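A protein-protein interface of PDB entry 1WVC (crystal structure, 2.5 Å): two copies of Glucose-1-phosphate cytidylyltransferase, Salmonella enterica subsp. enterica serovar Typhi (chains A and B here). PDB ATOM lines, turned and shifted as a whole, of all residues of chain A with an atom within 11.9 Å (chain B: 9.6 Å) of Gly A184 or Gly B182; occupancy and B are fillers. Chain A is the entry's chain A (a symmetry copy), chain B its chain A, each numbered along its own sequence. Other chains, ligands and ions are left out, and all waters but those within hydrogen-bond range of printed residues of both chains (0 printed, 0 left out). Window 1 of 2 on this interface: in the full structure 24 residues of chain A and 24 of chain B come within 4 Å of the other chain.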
ATOM      1  N   ALA A 156       2.140 -35.053 -11.967  1.00  0.00           N
ATOM      2  CA  ALA A 156       3.199 -34.096 -11.888  1.00  0.00           C
ATOM      3  C   ALA A 156       3.992 -34.267 -13.144  1.00  0.00           C
ATOM      4  O   ALA A 156       4.281 -35.387 -13.572  1.00  0.00           O
ATOM      5  CB  ALA A 156       4.024 -34.325 -10.640  1.00  0.00           C
ATOM      6  N   THR A 157       4.315 -33.147 -13.739  1.00  0.00           N
ATOM      7  CA  THR A 157       5.063 -33.204 -14.956  1.00  0.00           C
ATOM      8  C   THR A 157       6.131 -32.155 -15.015  1.00  0.00           C
ATOM      9  O   THR A 157       6.268 -31.234 -14.198  1.00  0.00           O
ATOM     10  CB  THR A 157       4.138 -32.943 -16.179  1.00  0.00           C
ATOM     11  OG1 THR A 157       3.815 -31.570 -16.242  1.00  0.00           O
ATOM     12  CG2 THR A 157       2.836 -33.710 -16.050  1.00  0.00           C
ATOM     13  N   PHE A 158       6.882 -32.325 -16.063  1.00  0.00           N
ATOM     14  CA  PHE A 158       7.880 -31.361 -16.300  1.00  0.00           C
ATOM     15  C   PHE A 158       7.204 -30.481 -17.286  1.00  0.00           C
ATOM     16  O   PHE A 158       6.409 -30.879 -18.145  1.00  0.00           O
ATOM     17  CB  PHE A 158       9.154 -31.874 -16.941  1.00  0.00           C
ATOM     18  CG  PHE A 158       9.955 -32.598 -15.930  1.00  0.00           C
ATOM     19  CD1 PHE A 158      10.137 -33.973 -16.057  1.00  0.00           C
ATOM     20  CD2 PHE A 158      10.499 -31.925 -14.835  1.00  0.00           C
ATOM     21  CE1 PHE A 158      10.881 -34.678 -15.113  1.00  0.00           C
ATOM     22  CE2 PHE A 158      11.238 -32.617 -13.875  1.00  0.00           C
ATOM     23  CZ  PHE A 158      11.428 -33.991 -14.028  1.00  0.00           C
ATOM     24  N   PRO A 159       7.557 -29.272 -17.109  1.00  0.00           N
ATOM     25  CA  PRO A 159       7.112 -28.161 -17.890  1.00  0.00           C
ATOM     26  C   PRO A 159       7.955 -28.008 -19.161  1.00  0.00           C
ATOM     27  O   PRO A 159       9.027 -28.584 -19.317  1.00  0.00           O
ATOM     28  CB  PRO A 159       7.426 -26.963 -16.997  1.00  0.00           C
ATOM     29  CG  PRO A 159       8.338 -27.455 -15.876  1.00  0.00           C
ATOM     30  CD  PRO A 159       8.183 -28.956 -15.813  1.00  0.00           C
ATOM     31  N   ALA A 165      16.804 -23.609 -19.439  1.00  0.00           N
ATOM     32  CA  ALA A 165      17.217 -24.560 -18.399  1.00  0.00           C
ATOM     33  C   ALA A 165      18.659 -25.036 -18.485  1.00  0.00           C
ATOM     34  O   ALA A 165      19.087 -25.540 -19.528  1.00  0.00           O
ATOM     35  CB  ALA A 165      16.255 -25.738 -18.342  1.00  0.00           C
ATOM     36  N   LEU A 166      19.384 -24.880 -17.362  1.00  0.00           N
ATOM     37  CA  LEU A 166      20.793 -25.250 -17.275  1.00  0.00           C
ATOM     38  C   LEU A 166      21.224 -26.408 -16.395  1.00  0.00           C
ATOM     39  O   LEU A 166      20.532 -26.895 -15.499  1.00  0.00           O
ATOM     40  CB  LEU A 166      21.701 -24.047 -16.921  1.00  0.00           C
ATOM     41  CG  LEU A 166      20.998 -22.692 -16.805  1.00  0.00           C
ATOM     42  CD1 LEU A 166      21.615 -21.889 -15.664  1.00  0.00           C
ATOM     43  CD2 LEU A 166      21.155 -21.905 -18.103  1.00  0.00           C
ATOM     44  N   ILE A 168      24.164 -26.920 -14.074  1.00  0.00           N
ATOM     45  CA  ILE A 168      25.149 -26.244 -13.264  1.00  0.00           C
ATOM     46  C   ILE A 168      25.611 -27.081 -12.122  1.00  0.00           C
ATOM     47  O   ILE A 168      24.809 -27.499 -11.276  1.00  0.00           O
ATOM     48  CB  ILE A 168      24.720 -24.912 -12.656  1.00  0.00           C
ATOM     49  CG1 ILE A 168      23.676 -24.165 -13.469  1.00  0.00           C
ATOM     50  CG2 ILE A 168      25.931 -24.022 -12.376  1.00  0.00           C
ATOM     51  CD1 ILE A 168      23.124 -23.010 -12.650  1.00  0.00           C
ATOM     52  N   GLN A 177      20.026 -27.292 -21.315  1.00  0.00           N
ATOM     53  CA  GLN A 177      19.024 -28.352 -21.476  1.00  0.00           C
ATOM     54  C   GLN A 177      17.592 -27.875 -21.758  1.00  0.00           C
ATOM     55  O   GLN A 177      16.652 -28.688 -21.818  1.00  0.00           O
ATOM     56  CB  GLN A 177      19.022 -29.276 -20.236  1.00  0.00           C
ATOM     57  CG  GLN A 177      20.373 -29.960 -19.951  1.00  0.00           C
ATOM     58  CD  GLN A 177      20.345 -30.783 -18.668  1.00  0.00           C
ATOM     59  OE1 GLN A 177      21.095 -31.767 -18.516  1.00  0.00           O
ATOM     60  NE2 GLN A 177      19.471 -30.378 -17.737  1.00  0.00           N
ATOM     61  N   LYS A 181      14.207 -28.829 -16.344  1.00  0.00           N
ATOM     62  CA  LYS A 181      13.896 -29.213 -14.969  1.00  0.00           C
ATOM     63  C   LYS A 181      14.704 -30.412 -14.431  1.00  0.00           C
ATOM     64  O   LYS A 181      14.973 -31.391 -15.139  1.00  0.00           O
ATOM     65  CB  LYS A 181      12.402 -29.393 -14.804  1.00  0.00           C
ATOM     66  N   GLY A 182      15.039 -30.329 -13.130  1.00  0.00           N
ATOM     67  CA  GLY A 182      15.887 -31.347 -12.552  1.00  0.00           C
ATOM     68  C   GLY A 182      15.205 -32.196 -11.492  1.00  0.00           C
ATOM     69  O   GLY A 182      14.897 -33.388 -11.700  1.00  0.00           O
ATOM     70  N   ASP A 183      14.947 -31.641 -10.345  1.00  0.00           N
ATOM     71  CA  ASP A 183      14.485 -32.506  -9.446  1.00  0.00           C
ATOM     72  C   ASP A 183      13.295 -32.281  -8.702  1.00  0.00           C
ATOM     73  O   ASP A 183      12.569 -33.245  -8.542  1.00  0.00           O
ATOM     74  CB  ASP A 183      15.272 -32.821  -8.196  1.00  0.00           C
ATOM     75  CG  ASP A 183      15.547 -31.664  -7.248  1.00  0.00           C
ATOM     76  OD1 ASP A 183      15.097 -30.483  -7.491  1.00  0.00           O
ATOM     77  OD2 ASP A 183      16.260 -31.932  -6.203  1.00  0.00           O
ATOM     78  N   GLY A 184      13.144 -31.049  -8.204  1.00  0.00           N
ATOM     79  CA  GLY A 184      11.949 -30.598  -7.367  1.00  0.00           C
ATOM     80  C   GLY A 184      11.275 -29.391  -8.197  1.00  0.00           C
ATOM     81  O   GLY A 184      10.778 -28.327  -7.670  1.00  0.00           O
ATOM     82  N   ALA A 185      11.389 -29.763  -9.447  1.00  0.00           N
ATOM     83  CA  ALA A 185      11.093 -29.054 -10.668  1.00  0.00           C
ATOM     84  C   ALA A 185       9.898 -29.598 -11.473  1.00  0.00           C
ATOM     85  O   ALA A 185       9.873 -29.572 -12.714  1.00  0.00           O
ATOM     86  CB  ALA A 185      12.344 -29.221 -11.536  1.00  0.00           C
ATOM     87  N   MET A 186       8.886 -30.096 -10.832  1.00  0.00           N
ATOM     88  CA  MET A 186       7.754 -30.579 -11.610  1.00  0.00           C
ATOM     89  C   MET A 186       6.556 -29.705 -11.346  1.00  0.00           C
ATOM     90  O   MET A 186       6.568 -28.884 -10.424  1.00  0.00           O
ATOM     91  CB  MET A 186       7.414 -32.018 -11.276  1.00  0.00           C
ATOM     92  CG  MET A 186       8.492 -32.977 -11.737  1.00  0.00           C
ATOM     93  SD  MET A 186       8.059 -34.668 -11.458  1.00  0.00           S
ATOM     94  CE  MET A 186       7.495 -35.308 -13.022  1.00  0.00           C
ATOM     95  N   ILE A 187       5.574 -29.893 -12.210  1.00  0.00           N
ATOM     96  CA  ILE A 187       4.376 -29.123 -12.064  1.00  0.00           C
ATOM     97  C   ILE A 187       3.163 -29.988 -12.201  1.00  0.00           C
ATOM     98  O   ILE A 187       3.217 -31.180 -12.527  1.00  0.00           O
ATOM     99  CB  ILE A 187       4.283 -28.033 -13.102  1.00  0.00           C
ATOM    100  CG1 ILE A 187       4.240 -28.665 -14.484  1.00  0.00           C
ATOM    101  CG2 ILE A 187       5.491 -27.136 -12.978  1.00  0.00           C
ATOM    102  CD1 ILE A 187       3.555 -27.780 -15.516  1.00  0.00           C
ATOM    103  N   ASN A 188       2.066 -29.317 -11.942  1.00  0.00           N
ATOM    104  CA  ASN A 188       0.788 -29.924 -12.055  1.00  0.00           C
ATOM    105  C   ASN A 188       0.396 -29.824 -13.529  1.00  0.00           C
ATOM    106  O   ASN A 188       0.248 -28.717 -14.074  1.00  0.00           O
ATOM    107  CB  ASN A 188      -0.209 -29.189 -11.158  1.00  0.00           C
ATOM    108  CG  ASN A 188      -1.655 -29.335 -11.602  1.00  0.00           C
ATOM    109  OD1 ASN A 188      -2.098 -30.406 -12.068  1.00  0.00           O
ATOM    110  ND2 ASN A 188      -2.402 -28.248 -11.439  1.00  0.00           N
ATOM    111  N   ALA A 225       0.951 -37.326  -5.844  1.00  0.00           N
ATOM    112  CA  ALA A 225       1.431 -36.894  -7.131  1.00  0.00           C
ATOM    113  C   ALA A 225       1.999 -38.024  -7.961  1.00  0.00           C
ATOM    114  O   ALA A 225       2.950 -38.724  -7.587  1.00  0.00           O
ATOM    115  CB  ALA A 225       2.408 -35.738  -7.027  1.00  0.00           C
ATOM    116  N   GLU A 227       4.107 -39.006 -10.863  1.00  0.00           N
ATOM    117  CA  GLU A 227       5.213 -38.441 -11.643  1.00  0.00           C
ATOM    118  C   GLU A 227       5.332 -38.913 -13.082  1.00  0.00           C
ATOM    119  O   GLU A 227       5.506 -40.097 -13.363  1.00  0.00           O
ATOM    120  CB  GLU A 227       6.600 -38.554 -10.978  1.00  0.00           C
ATOM    121  CG  GLU A 227       6.679 -38.201  -9.475  1.00  0.00           C
ATOM    122  CD  GLU A 227       8.095 -38.270  -8.934  1.00  0.00           C
ATOM    123  OE1 GLU A 227       9.090 -38.318  -9.652  1.00  0.00           O
ATOM    124  OE2 GLU A 227       8.143 -38.289  -7.619  1.00  0.00           O
ATOM    125  N   HIS A 228       5.265 -37.947 -13.992  1.00  0.00           N
ATOM    126  CA  HIS A 228       5.386 -38.207 -15.411  1.00  0.00           C
ATOM    127  C   HIS A 228       6.616 -37.479 -15.921  1.00  0.00           C
ATOM    128  O   HIS A 228       6.702 -36.246 -15.896  1.00  0.00           O
ATOM    129  CB  HIS A 228       4.095 -37.845 -16.212  1.00  0.00           C
ATOM    130  CG  HIS A 228       4.216 -37.860 -17.727  1.00  0.00           C
ATOM    131  ND1 HIS A 228       4.212 -39.049 -18.462  1.00  0.00           N
ATOM    132  CD2 HIS A 228       4.338 -36.823 -18.610  1.00  0.00           C
ATOM    133  CE1 HIS A 228       4.335 -38.721 -19.747  1.00  0.00           C
ATOM    134  NE2 HIS A 228       4.405 -37.393 -19.864  1.00  0.00           N
ATOM    135  N   PRO A 229       7.577 -38.269 -16.373  1.00  0.00           N
ATOM    136  CA  PRO A 229       8.836 -37.757 -16.898  1.00  0.00           C
ATOM    137  C   PRO A 229       8.756 -37.428 -18.402  1.00  0.00           C
ATOM    138  O   PRO A 229       9.423 -36.523 -18.929  1.00  0.00           O
ATOM    139  CB  PRO A 229       9.840 -38.898 -16.686  1.00  0.00           C
ATOM    140  CG  PRO A 229       9.011 -40.167 -16.521  1.00  0.00           C
ATOM    141  CD  PRO A 229       7.577 -39.746 -16.220  1.00  0.00           C
ATOM    142  N   THR B 157      19.153 -17.904 -12.890  1.00  0.00           N
ATOM    143  CA  THR B 157      18.057 -17.484 -12.075  1.00  0.00           C
ATOM    144  C   THR B 157      16.937 -18.480 -12.076  1.00  0.00           C
ATOM    145  O   THR B 157      16.871 -19.475 -12.811  1.00  0.00           O
ATOM    146  CB  THR B 157      17.450 -16.157 -12.615  1.00  0.00           C
ATOM    147  OG1 THR B 157      16.703 -16.420 -13.783  1.00  0.00           O
ATOM    148  CG2 THR B 157      18.542 -15.172 -12.985  1.00  0.00           C
ATOM    149  N   PHE B 158      16.022 -18.140 -11.217  1.00  0.00           N
ATOM    150  CA  PHE B 158      14.862 -18.936 -11.166  1.00  0.00           C
ATOM    151  C   PHE B 158      13.936 -18.154 -12.024  1.00  0.00           C
ATOM    152  O   PHE B 158      13.925 -16.920 -12.093  1.00  0.00           O
ATOM    153  CB  PHE B 158      14.216 -19.074  -9.802  1.00  0.00           C
ATOM    154  CG  PHE B 158      15.013 -20.008  -8.975  1.00  0.00           C
ATOM    155  CD1 PHE B 158      15.691 -19.525  -7.858  1.00  0.00           C
ATOM    156  CD2 PHE B 158      15.119 -21.355  -9.322  1.00  0.00           C
ATOM    157  CE1 PHE B 158      16.454 -20.383  -7.068  1.00  0.00           C
ATOM    158  CE2 PHE B 158      15.887 -22.226  -8.547  1.00  0.00           C
ATOM    159  CZ  PHE B 158      16.543 -21.731  -7.420  1.00  0.00           C
ATOM    160  N   PRO B 159      13.172 -18.937 -12.672  1.00  0.00           N
ATOM    161  CA  PRO B 159      12.150 -18.524 -13.581  1.00  0.00           C
ATOM    162  C   PRO B 159      10.849 -18.203 -12.837  1.00  0.00           C
ATOM    163  O   PRO B 159      10.653 -18.536 -11.672  1.00  0.00           O
ATOM    164  CB  PRO B 159      11.894 -19.783 -14.407  1.00  0.00           C
ATOM    165  CG  PRO B 159      12.577 -20.946 -13.692  1.00  0.00           C
ATOM    166  CD  PRO B 159      13.599 -20.345 -12.757  1.00  0.00           C
ATOM    167  N   GLY B 164       3.008 -23.761 -12.059  1.00  0.00           N
ATOM    168  CA  GLY B 164       2.307 -24.679 -11.159  1.00  0.00           C
ATOM    169  C   GLY B 164       3.274 -25.633 -10.472  1.00  0.00           C
ATOM    170  O   GLY B 164       3.056 -26.854 -10.508  1.00  0.00           O
ATOM    171  N   ALA B 165       4.331 -25.021  -9.875  1.00  0.00           N
ATOM    172  CA  ALA B 165       5.446 -25.654  -9.158  1.00  0.00           C
ATOM    173  C   ALA B 165       5.084 -26.299  -7.830  1.00  0.00           C
ATOM    174  O   ALA B 165       4.508 -25.643  -6.954  1.00  0.00           O
ATOM    175  CB  ALA B 165       6.600 -24.676  -8.994  1.00  0.00           C
ATOM    176  N   LEU B 166       5.451 -27.588  -7.696  1.00  0.00           N
ATOM    177  CA  LEU B 166       5.154 -28.372  -6.502  1.00  0.00           C
ATOM    178  C   LEU B 166       6.279 -28.828  -5.592  1.00  0.00           C
ATOM    179  O   LEU B 166       7.468 -28.856  -5.915  1.00  0.00           O
ATOM    180  CB  LEU B 166       4.286 -29.616  -6.810  1.00  0.00           C
ATOM    181  CG  LEU B 166       3.828 -29.767  -8.263  1.00  0.00           C
ATOM    182  CD1 LEU B 166       3.855 -31.238  -8.661  1.00  0.00           C
ATOM    183  CD2 LEU B 166       2.404 -29.240  -8.422  1.00  0.00           C
ATOM    184  N   ASP B 167       5.796 -29.213  -4.412  1.00  0.00           N
ATOM    185  CA  ASP B 167       6.554 -29.743  -3.306  1.00  0.00           C
ATOM    186  C   ASP B 167       6.127 -31.190  -3.172  1.00  0.00           C
ATOM    187  O   ASP B 167       5.066 -31.485  -2.589  1.00  0.00           O
ATOM    188  CB  ASP B 167       6.253 -29.015  -1.989  1.00  0.00           C
ATOM    189  CG  ASP B 167       7.125 -29.518  -0.876  1.00  0.00           C
ATOM    190  OD1 ASP B 167       8.141 -30.165  -1.075  1.00  0.00           O
ATOM    191  OD2 ASP B 167       6.668 -29.197   0.308  1.00  0.00           O
ATOM    192  N   ILE B 168       6.952 -32.064  -3.755  1.00  0.00           N
ATOM    193  CA  ILE B 168       6.682 -33.482  -3.742  1.00  0.00           C
ATOM    194  C   ILE B 168       7.775 -34.259  -3.094  1.00  0.00           C
ATOM    195  O   ILE B 168       8.933 -34.210  -3.530  1.00  0.00           O
ATOM    196  CB  ILE B 168       6.457 -34.136  -5.102  1.00  0.00           C
ATOM    197  CG1 ILE B 168       5.881 -33.202  -6.154  1.00  0.00           C
ATOM    198  CG2 ILE B 168       5.605 -35.398  -4.969  1.00  0.00           C
ATOM    199  CD1 ILE B 168       5.958 -33.864  -7.519  1.00  0.00           C
ATOM    200  N   GLN B 169       7.327 -34.980  -2.070  1.00  0.00           N
ATOM    201  CA  GLN B 169       8.134 -35.857  -1.247  1.00  0.00           C
ATOM    202  C   GLN B 169       7.444 -37.205  -1.114  1.00  0.00           C
ATOM    203  O   GLN B 169       6.295 -37.278  -0.688  1.00  0.00           O
ATOM    204  CB  GLN B 169       8.411 -35.238   0.140  1.00  0.00           C
ATOM    205  CG  GLN B 169       9.863 -34.736   0.268  1.00  0.00           C
ATOM    206  CD  GLN B 169       9.977 -33.426   1.021  1.00  0.00           C
ATOM    207  OE1 GLN B 169       9.623 -33.331   2.209  1.00  0.00           O
ATOM    208  NE2 GLN B 169      10.485 -32.410   0.330  1.00  0.00           N
ATOM    209  N   SER B 175       2.898 -29.303  -1.059  1.00  0.00           N
ATOM    210  CA  SER B 175       2.393 -27.959  -1.272  1.00  0.00           C
ATOM    211  C   SER B 175       2.652 -27.462  -2.671  1.00  0.00           C
ATOM    212  O   SER B 175       3.524 -27.974  -3.360  1.00  0.00           O
ATOM    213  CB  SER B 175       3.081 -26.960  -0.371  1.00  0.00           C
ATOM    214  OG  SER B 175       3.908 -26.115  -1.167  1.00  0.00           O
ATOM    215  N   GLN B 177       3.982 -24.318  -4.694  1.00  0.00           N
ATOM    216  CA  GLN B 177       4.932 -23.204  -4.592  1.00  0.00           C
ATOM    217  C   GLN B 177       5.040 -22.308  -5.833  1.00  0.00           C
ATOM    218  O   GLN B 177       5.883 -21.394  -5.886  1.00  0.00           O
ATOM    219  CB  GLN B 177       6.337 -23.735  -4.219  1.00  0.00           C
ATOM    220  CG  GLN B 177       6.390 -24.509  -2.887  1.00  0.00           C
ATOM    221  CD  GLN B 177       7.772 -25.090  -2.612  1.00  0.00           C
ATOM    222  OE1 GLN B 177       8.167 -25.293  -1.447  1.00  0.00           O
ATOM    223  NE2 GLN B 177       8.515 -25.360  -3.693  1.00  0.00           N
ATOM    224  N   LYS B 181      10.681 -23.695  -8.652  1.00  0.00           N
ATOM    225  CA  LYS B 181      11.974 -24.330  -8.897  1.00  0.00           C
ATOM    226  C   LYS B 181      12.737 -24.760  -7.627  1.00  0.00           C
ATOM    227  O   LYS B 181      12.744 -24.068  -6.600  1.00  0.00           O
ATOM    228  CB  LYS B 181      12.812 -23.467  -9.817  1.00  0.00           C
ATOM    229  N   GLY B 182      13.428 -25.908  -7.746  1.00  0.00           N
ATOM    230  CA  GLY B 182      14.092 -26.458  -6.585  1.00  0.00           C
ATOM    231  C   GLY B 182      15.608 -26.475  -6.684  1.00  0.00           C
ATOM    232  O   GLY B 182      16.322 -25.703  -6.011  1.00  0.00           O
ATOM    233  N   ASP B 183      16.153 -27.326  -7.503  1.00  0.00           N
ATOM    234  CA  ASP B 183      17.479 -27.358  -7.407  1.00  0.00           C
ATOM    235  C   ASP B 183      18.336 -27.237  -8.534  1.00  0.00           C
ATOM    236  O   ASP B 183      19.331 -26.552  -8.384  1.00  0.00           O
ATOM    237  CB  ASP B 183      18.193 -28.600  -6.929  1.00  0.00           C
ATOM    238  CG  ASP B 183      18.015 -29.858  -7.764  1.00  0.00           C
ATOM    239  OD1 ASP B 183      17.316 -29.847  -8.846  1.00  0.00           O
ATOM    240  OD2 ASP B 183      18.592 -30.928  -7.325  1.00  0.00           O
ATOM    241  N   GLY B 184      17.983 -27.947  -9.612  1.00  0.00           N
ATOM    242  CA  GLY B 184      18.766 -27.971 -10.922  1.00  0.00           C
ATOM    243  C   GLY B 184      17.746 -27.420 -12.043  1.00  0.00           C
ATOM    244  O   GLY B 184      17.659 -27.877 -13.243  1.00  0.00           O
ATOM    245  N   ALA B 185      17.080 -26.475 -11.428  1.00  0.00           N
ATOM    246  CA  ALA B 185      15.943 -25.697 -11.857  1.00  0.00           C
ATOM    247  C   ALA B 185      16.223 -24.203 -12.105  1.00  0.00           C
ATOM    248  O   ALA B 185      15.376 -23.326 -11.866  1.00  0.00           O
ATOM    249  CB  ALA B 185      14.942 -25.790 -10.701  1.00  0.00           C
ATOM    250  N   MET B 186      17.377 -23.854 -12.582  1.00  0.00           N
ATOM    251  CA  MET B 186      17.611 -22.438 -12.837  1.00  0.00           C
ATOM    252  C   MET B 186      17.750 -22.214 -14.319  1.00  0.00           C
ATOM    253  O   MET B 186      17.868 -23.170 -15.092  1.00  0.00           O
ATOM    254  CB  MET B 186      18.855 -21.938 -12.130  1.00  0.00           C
ATOM    255  CG  MET B 186      18.684 -21.920 -10.625  1.00  0.00           C
ATOM    256  SD  MET B 186      20.083 -21.231  -9.793  1.00  0.00           S
ATOM    257  CE  MET B 186      19.647 -19.554  -9.379  1.00  0.00           C
ATOM    258  N   ILE B 187      17.684 -20.939 -14.662  1.00  0.00           N
ATOM    259  CA  ILE B 187      17.807 -20.594 -16.044  1.00  0.00           C
ATOM    260  C   ILE B 187      18.742 -19.440 -16.228  1.00  0.00           C
ATOM    261  O   ILE B 187      19.226 -18.806 -15.283  1.00  0.00           O
ATOM    262  CB  ILE B 187      16.478 -20.209 -16.643  1.00  0.00           C
ATOM    263  CG1 ILE B 187      15.946 -18.980 -15.924  1.00  0.00           C
ATOM    264  CG2 ILE B 187      15.517 -21.361 -16.484  1.00  0.00           C
ATOM    265  CD1 ILE B 187      14.989 -18.162 -16.780  1.00  0.00           C
ATOM    266  N   GLU B 227      24.761 -17.646  -9.553  1.00  0.00           N
ATOM    267  CA  GLU B 227      23.432 -17.980  -9.029  1.00  0.00           C
ATOM    268  C   GLU B 227      22.698 -16.869  -8.299  1.00  0.00           C
ATOM    269  O   GLU B 227      23.157 -16.343  -7.288  1.00  0.00           O
ATOM    270  CB  GLU B 227      23.380 -19.252  -8.159  1.00  0.00           C
ATOM    271  CG  GLU B 227      24.149 -20.484  -8.684  1.00  0.00           C
ATOM    272  CD  GLU B 227      23.974 -21.703  -7.797  1.00  0.00           C
ATOM    273  OE1 GLU B 227      23.108 -21.788  -6.932  1.00  0.00           O
ATOM    274  OE2 GLU B 227      24.856 -22.650  -8.042  1.00  0.00           O
ATOM    275  N   PRO B 229      19.152 -16.164  -6.505  1.00  0.00           N
ATOM    276  CA  PRO B 229      17.966 -16.752  -5.895  1.00  0.00           C
ATOM    277  C   PRO B 229      16.780 -15.767  -5.849  1.00  0.00           C
ATOM    278  O   PRO B 229      15.596 -16.136  -5.915  1.00  0.00           O
ATOM    279  CB  PRO B 229      18.391 -17.094  -4.462  1.00  0.00           C
ATOM    280  CG  PRO B 229      19.619 -16.238  -4.168  1.00  0.00           C
ATOM    281  CD  PRO B 229      20.156 -15.730  -5.501  1.00  0.00           C
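Leu B166 touches Ala A156. Ala A156 touches Ile B168 (CB to CD1, 3.7 Å). Ala A165 touches Met B186 (CA to O, 3.6 Å). Ala A165 touches Ile B187. Leu A166 touches Gly B184 (O to O, 3.8 Å). Ile B187 touches Leu A166 (C to CD1, 3.8 Å). N of Gly A182 touches O of Gly B184, at 3.6 Å. O of Gly A184 touches N of Gly B182 (3.6 Å). Ile A187 touches Gly B164. Leu B166 touches Asn A188 (CD2 to N, 3.5 Å).
Of the printed residues of chain B, Gly A184 touches Leu B166 (3.8 Å) and Gly B182 (3.6 Å). Printed residues of chain A within 4 Å of Gly B182: Gly A184. Gly A182 touches just one residue of chain B: Gly B184. Asp A183 touches just one residue of chain B: Asp B183 (2.7 Å). Of chain A, only Met A186 (3.6 Å) and Ile A187 (3.9 Å) come within 4 Å of Ala B165. Asp B183 touches just one residue of chain A: Asp A183 (2.7 Å). Of chain A, only Leu A166 (3.8 Å) and Gly A182 (3.6 Å) come within 4 Å of Gly B184. Printed residues of chain B within 4 Å of Ala A225: Ile B168. Printed residues of chain A within 4 Å of Ile B168: Ala A156 and Ala A225. The nearest residue of chain B that does not touch Gly A184 is Lys B181 (4.1 Å). The nearest residue of chain A that does not touch Gly B182 is Asp A183 (4.1 Å). The nearest printed residue of chain A that does not touch Met B186 is Ile A168 (4.4 Å).
N of His A228 lies within hydrogen-bond range of O of Ala A156 (2.8 Å). The backbone NH (N) of Ile A187 is in hydrogen-bond range of the backbone carbonyl oxygen (O) of Thr A157, 2.5 Å away. The backbone NH (N) of Gln A177 lies within hydrogen-bond range of the backbone carbonyl oxygen (O) of Ala A165, 2.7 Å away. The backbone carbonyl oxygen of Thr B157 sits at hydrogen-bond distance from the backbone NH of Ile B187, 2.5 Å away. O of Ala B165 lies within hydrogen-bond range of N of Gln B177, at 2.7 Å.
Ala A165 touches Met B186, and with the chains exchanged Met A186 touches Ala B165. Ala A165 touches Ile B187, and with the chains exchanged Ile A187 touches Ala B165. Leu A166 touches Gly B184, and with the chains exchanged Gly A184 touches Leu B166. Leu A166 touches Met B186, and with the chains exchanged Met A186 touches Leu B166. 16 positions are printed for both chains. Of the 19 pairs that touch across the chains among the printed residues, 13 have their exchanged pair printed and touching as well.
O of Met B186 is in hydrogen-bond range of N of Leu A166 (3.2 Å). The backbone NH of Asp A183 lies close to the side-chain carboxylate of Asp B183, 3.3 Å away. N of Leu B166 is in hydrogen-bond range of O of Met A186. The backbone NH (N) of Asn A188 lies within hydrogen-bond range of the backbone carbonyl oxygen (O) of Gly B164 (3.0 Å).
Printed residues of chain B that touch a printed residue of chain A: Gly B164, Ala B165, Leu B166, Ile B168, Gly B182, Asp B183, Gly B184, Met B186 and Ile B187. Hydrophobic or aromatic side chains of chain B that line the printed part of chain A: Leu B166, Ile B168 and Ile B187. Hydrophobic or aromatic side chains of chain A within 4 Å of the printed part of chain B: Ala A156, Leu A166, Ile A187 and Ala A225. Among the printed residues, 19 pairs touch across the chains. Among the printed residues, no Asp or Glu carboxylate lies within 4 Å of a Lys or Arg side-chain nitrogen of the other chain.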
